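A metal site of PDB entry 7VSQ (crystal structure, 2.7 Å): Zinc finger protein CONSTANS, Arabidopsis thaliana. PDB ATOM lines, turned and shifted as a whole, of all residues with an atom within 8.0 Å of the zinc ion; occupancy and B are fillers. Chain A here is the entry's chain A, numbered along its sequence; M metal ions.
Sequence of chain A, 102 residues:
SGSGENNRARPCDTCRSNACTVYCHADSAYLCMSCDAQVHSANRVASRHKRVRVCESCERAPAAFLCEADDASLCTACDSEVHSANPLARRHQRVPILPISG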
ATOM      1  N   TYR A  23       7.866  24.714 -20.329  1.00  0.00           N
ATOM      2  CA  TYR A  23       8.956  23.937 -19.779  1.00  0.00           C
ATOM      3  C   TYR A  23       8.538  22.497 -19.548  1.00  0.00           C
ATOM      4  O   TYR A  23       7.492  22.224 -18.925  1.00  0.00           O
ATOM      5  CB  TYR A  23       9.459  24.562 -18.483  1.00  0.00           C
ATOM      6  CG  TYR A  23      10.529  23.766 -17.767  1.00  0.00           C
ATOM      7  CD1 TYR A  23      11.709  23.425 -18.408  1.00  0.00           C
ATOM      8  CD2 TYR A  23      10.386  23.404 -16.435  1.00  0.00           C
ATOM      9  CE1 TYR A  23      12.702  22.713 -17.760  1.00  0.00           C
ATOM     10  CE2 TYR A  23      11.365  22.699 -15.771  1.00  0.00           C
ATOM     11  CZ  TYR A  23      12.524  22.359 -16.438  1.00  0.00           C
ATOM     12  OH  TYR A  23      13.517  21.647 -15.789  1.00  0.00           O
ATOM     13  N   CYS A  24       9.349  21.566 -20.060  1.00  0.00           N
ATOM     14  CA  CYS A  24       9.187  20.154 -19.751  1.00  0.00           C
ATOM     15  C   CYS A  24      10.317  19.731 -18.825  1.00  0.00           C
ATOM     16  O   CYS A  24      11.493  19.871 -19.155  1.00  0.00           O
ATOM     17  CB  CYS A  24       9.175  19.282 -20.994  1.00  0.00           C
ATOM     18  SG  CYS A  24       8.873  17.535 -20.642  1.00  0.00           S
ATOM     19  N   HIS A  25       9.949  19.236 -17.645  1.00  0.00           N
ATOM     20  CA  HIS A  25      10.913  18.810 -16.649  1.00  0.00           C
ATOM     21  C   HIS A  25      11.584  17.483 -16.992  1.00  0.00           C
ATOM     22  O   HIS A  25      12.776  17.311 -16.786  1.00  0.00           O
ATOM     23  CB  HIS A  25      10.230  18.668 -15.285  1.00  0.00           C
ATOM     24  CG  HIS A  25      11.155  18.275 -14.179  1.00  0.00           C
ATOM     25  ND1 HIS A  25      10.782  17.431 -13.157  1.00  0.00           N
ATOM     26  CD2 HIS A  25      12.415  18.684 -13.894  1.00  0.00           C
ATOM     27  CE1 HIS A  25      11.793  17.297 -12.319  1.00  0.00           C
ATOM     28  NE2 HIS A  25      12.798  18.047 -12.742  1.00  0.00           N
ATOM     29  N   ALA A  26      10.786  16.551 -17.500  1.00  0.00           N
ATOM     30  CA  ALA A  26      11.278  15.236 -17.890  1.00  0.00           C
ATOM     31  C   ALA A  26      12.329  15.350 -18.973  1.00  0.00           C
ATOM     32  O   ALA A  26      13.393  14.728 -18.910  1.00  0.00           O
ATOM     33  CB  ALA A  26      10.132  14.365 -18.361  1.00  0.00           C
ATOM     34  N   ASP A  27      12.033  16.161 -19.965  1.00  0.00           N
ATOM     35  CA  ASP A  27      12.970  16.475 -21.021  1.00  0.00           C
ATOM     36  C   ASP A  27      13.978  17.486 -20.508  1.00  0.00           C
ATOM     37  O   ASP A  27      15.038  17.662 -21.095  1.00  0.00           O
ATOM     38  CB  ASP A  27      12.232  17.021 -22.240  1.00  0.00           C
ATOM     39  CG  ASP A  27      11.370  15.972 -22.935  1.00  0.00           C
ATOM     40  OD1 ASP A  27      11.821  14.801 -23.060  1.00  0.00           O
ATOM     41  OD2 ASP A  27      10.255  16.311 -23.364  1.00  0.00           O
ATOM     42  N   SER A  28      13.653  18.119 -19.382  1.00  0.00           N
ATOM     43  CA  SER A  28      14.489  19.150 -18.767  1.00  0.00           C
ATOM     44  C   SER A  28      14.881  20.213 -19.778  1.00  0.00           C
ATOM     45  O   SER A  28      16.026  20.663 -19.808  1.00  0.00           O
ATOM     46  CB  SER A  28      15.737  18.541 -18.117  1.00  0.00           C
ATOM     47  OG  SER A  28      16.242  17.421 -18.854  1.00  0.00           O
ATOM     48  N   ALA A  29      13.924  20.630 -20.600  1.00  0.00           N
ATOM     49  CA  ALA A  29      14.186  21.664 -21.593  1.00  0.00           C
ATOM     50  C   ALA A  29      12.996  22.606 -21.735  1.00  0.00           C
ATOM     51  O   ALA A  29      11.850  22.247 -21.466  1.00  0.00           O
ATOM     52  CB  ALA A  29      14.536  21.044 -22.943  1.00  0.00           C
ATOM     53  N   LEU A  31      10.744  24.980 -24.183  1.00  0.00           N
ATOM     54  CA  LEU A  31      10.377  24.957 -25.595  1.00  0.00           C
ATOM     55  C   LEU A  31       9.417  26.079 -25.999  1.00  0.00           C
ATOM     56  O   LEU A  31       8.780  26.704 -25.157  1.00  0.00           O
ATOM     57  CB  LEU A  31       9.744  23.612 -25.935  1.00  0.00           C
ATOM     58  CG  LEU A  31      10.776  22.483 -25.954  1.00  0.00           C
ATOM     59  CD1 LEU A  31      10.156  21.148 -26.334  1.00  0.00           C
ATOM     60  CD2 LEU A  31      11.945  22.837 -26.850  1.00  0.00           C
ATOM     61  N   ASP A  36       6.980  22.113 -28.696  1.00  0.00           N
ATOM     62  CA  ASP A  36       6.259  21.404 -27.643  1.00  0.00           C
ATOM     63  C   ASP A  36       5.288  20.376 -28.216  1.00  0.00           C
ATOM     64  O   ASP A  36       5.309  19.201 -27.845  1.00  0.00           O
ATOM     65  CB  ASP A  36       5.493  22.382 -26.768  1.00  0.00           C
ATOM     66  CG  ASP A  36       4.721  21.693 -25.674  1.00  0.00           C
ATOM     67  OD1 ASP A  36       5.369  21.212 -24.728  1.00  0.00           O
ATOM     68  OD2 ASP A  36       3.479  21.596 -25.783  1.00  0.00           O
ATOM     69  N   VAL A  39       7.316  17.476 -30.339  1.00  0.00           N
ATOM     70  CA  VAL A  39       8.155  16.581 -29.570  1.00  0.00           C
ATOM     71  C   VAL A  39       7.360  15.550 -28.791  1.00  0.00           C
ATOM     72  O   VAL A  39       7.745  14.383 -28.718  1.00  0.00           O
ATOM     73  CB  VAL A  39       9.043  17.387 -28.590  1.00  0.00           C
ATOM     74  CG1 VAL A  39       9.776  16.468 -27.641  1.00  0.00           C
ATOM     75  CG2 VAL A  39      10.005  18.272 -29.355  1.00  0.00           C
ATOM     76  N   HIS A  40       6.250  15.979 -28.227  1.00  0.00           N
ATOM     77  CA  HIS A  40       5.500  15.104 -27.330  1.00  0.00           C
ATOM     78  C   HIS A  40       4.331  14.412 -28.017  1.00  0.00           C
ATOM     79  O   HIS A  40       3.579  13.663 -27.387  1.00  0.00           O
ATOM     80  CB  HIS A  40       5.045  15.907 -26.118  1.00  0.00           C
ATOM     81  CG  HIS A  40       6.176  16.465 -25.301  1.00  0.00           C
ATOM     82  ND1 HIS A  40       7.076  17.381 -25.815  1.00  0.00           N
ATOM     83  CD2 HIS A  40       6.590  16.199 -24.043  1.00  0.00           C
ATOM     84  CE1 HIS A  40       7.968  17.674 -24.894  1.00  0.00           C
ATOM     85  NE2 HIS A  40       7.703  16.967 -23.810  1.00  0.00           N
ATOM     86  N   VAL A  45       4.742   7.855 -25.150  1.00  0.00           N
ATOM     87  CA  VAL A  45       5.471   8.113 -23.907  1.00  0.00           C
ATOM     88  C   VAL A  45       5.820   9.577 -23.746  1.00  0.00           C
ATOM     89  O   VAL A  45       5.814  10.109 -22.645  1.00  0.00           O
ATOM     90  CB  VAL A  45       6.774   7.292 -23.847  1.00  0.00           C
ATOM     91  CG1 VAL A  45       7.297   7.230 -22.423  1.00  0.00           C
ATOM     92  CG2 VAL A  45       6.530   5.910 -24.401  1.00  0.00           C
ATOM     93  N   ALA A  46       6.148  10.225 -24.865  1.00  0.00           N
ATOM     94  CA  ALA A  46       6.348  11.663 -24.880  1.00  0.00           C
ATOM     95  C   ALA A  46       5.019  12.366 -24.619  1.00  0.00           C
ATOM     96  O   ALA A  46       4.981  13.448 -24.042  1.00  0.00           O
ATOM     97  CB  ALA A  46       6.937  12.096 -26.207  1.00  0.00           C
ATOM     98  N   SER A  47       3.942  11.723 -25.045  1.00  0.00           N
ATOM     99  CA  SER A  47       2.572  12.201 -24.869  1.00  0.00           C
ATOM    100  C   SER A  47       2.227  12.382 -23.402  1.00  0.00           C
ATOM    101  O   SER A  47       1.416  13.232 -23.043  1.00  0.00           O
ATOM    102  CB  SER A  47       1.574  11.241 -25.515  1.00  0.00           C
ATOM    103  OG  SER A  47       1.103  10.305 -24.557  1.00  0.00           O
ATOM    104  N   ARG A  48       2.854  11.576 -22.550  1.00  0.00           N
ATOM    105  CA  ARG A  48       2.479  11.560 -21.146  1.00  0.00           C
ATOM    106  C   ARG A  48       3.441  12.415 -20.317  1.00  0.00           C
ATOM    107  O   ARG A  48       3.332  12.515 -19.098  1.00  0.00           O
ATOM    108  CB  ARG A  48       2.482  10.097 -20.658  1.00  0.00           C
ATOM    109  CG  ARG A  48       2.328   9.930 -19.169  1.00  0.00           C
ATOM    110  CD  ARG A  48       2.473   8.515 -18.653  1.00  0.00           C
ATOM    111  NE  ARG A  48       2.379   8.406 -17.190  1.00  0.00           N
ATOM    112  CZ  ARG A  48       1.528   9.063 -16.393  1.00  0.00           C
ATOM    113  NH1 ARG A  48       1.582   8.857 -15.081  1.00  0.00           N
ATOM    114  NH2 ARG A  48       0.597   9.890 -16.867  1.00  0.00           N
ATOM    115  N   HIS A  49       4.300  13.150 -20.997  1.00  0.00           N
ATOM    116  CA  HIS A  49       5.053  14.165 -20.293  1.00  0.00           C
ATOM    117  C   HIS A  49       4.077  15.194 -19.750  1.00  0.00           C
ATOM    118  O   HIS A  49       3.030  15.421 -20.337  1.00  0.00           O
ATOM    119  CB  HIS A  49       6.064  14.837 -21.204  1.00  0.00           C
ATOM    120  CG  HIS A  49       7.314  14.043 -21.394  1.00  0.00           C
ATOM    121  ND1 HIS A  49       8.183  14.261 -22.445  1.00  0.00           N
ATOM    122  CD2 HIS A  49       7.849  13.035 -20.660  1.00  0.00           C
ATOM    123  CE1 HIS A  49       9.199  13.416 -22.350  1.00  0.00           C
ATOM    124  NE2 HIS A  49       9.022  12.663 -21.273  1.00  0.00           N
ATOM    125  N   LYS A  50       4.395  15.812 -18.628  1.00  0.00           N
ATOM    126  CA  LYS A  50       3.571  16.910 -18.193  1.00  0.00           C
ATOM    127  C   LYS A  50       4.415  18.179 -18.177  1.00  0.00           C
ATOM    128  O   LYS A  50       5.536  18.233 -17.657  1.00  0.00           O
ATOM    129  CB  LYS A  50       2.928  16.634 -16.826  1.00  0.00           C
ATOM    130  CG  LYS A  50       1.515  16.135 -16.920  1.00  0.00           C
ATOM    131  CD  LYS A  50       0.659  17.162 -17.687  1.00  0.00           C
ATOM    132  CE  LYS A  50       0.818  18.594 -17.114  1.00  0.00           C
ATOM    133  NZ  LYS A  50       0.263  19.591 -18.068  1.00  0.00           N
ATOM    134  N   ARG A  51       3.833  19.196 -18.797  1.00  0.00           N
ATOM    135  CA  ARG A  51       4.537  20.409 -19.135  1.00  0.00           C
ATOM    136  C   ARG A  51       3.840  21.655 -18.600  1.00  0.00           C
ATOM    137  O   ARG A  51       2.624  21.820 -18.714  1.00  0.00           O
ATOM    138  CB  ARG A  51       4.724  20.466 -20.661  1.00  0.00           C
ATOM    139  CG  ARG A  51       5.222  19.123 -21.207  1.00  0.00           C
ATOM    140  CD  ARG A  51       5.404  19.086 -22.710  1.00  0.00           C
ATOM    141  NE  ARG A  51       4.193  19.299 -23.493  1.00  0.00           N
ATOM    142  CZ  ARG A  51       3.291  18.364 -23.745  1.00  0.00           C
ATOM    143  NH1 ARG A  51       3.450  17.142 -23.250  1.00  0.00           N
ATOM    144  NH2 ARG A  51       2.229  18.641 -24.483  1.00  0.00           N
HETATM  145 ZN    ZN M   1       8.729  16.189 -22.299  1.00  0.00          ZN
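The backbone carbonyl oxygen of His 40 is in hydrogen-bond range of the backbone NH of Ser 47. O of His 49 lies within hydrogen-bond range of NH1 of Arg 51 (3.4 Å). The backbone carbonyl oxygen of Cys 24 is in hydrogen-bond range of the backbone NH of Ala 29 (2.9 Å). The backbone carbonyl oxygen of Asp 36 is in hydrogen-bond range of a ring nitrogen (ND1) of His 40.
Within 4 Å of the zinc ion: Cys 24, Asp 27, His 40 and His 49.
The zinc ion is bound by the side-chain carboxylate (OD2) of Asp 27 (1.9 Å), a ring nitrogen (NE2) of His 40 (2.0 Å), a ring nitrogen (ND1) of His 49 (2.0 Å) and the side-chain sulfur (SG) of Cys 24 (2.1 Å).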
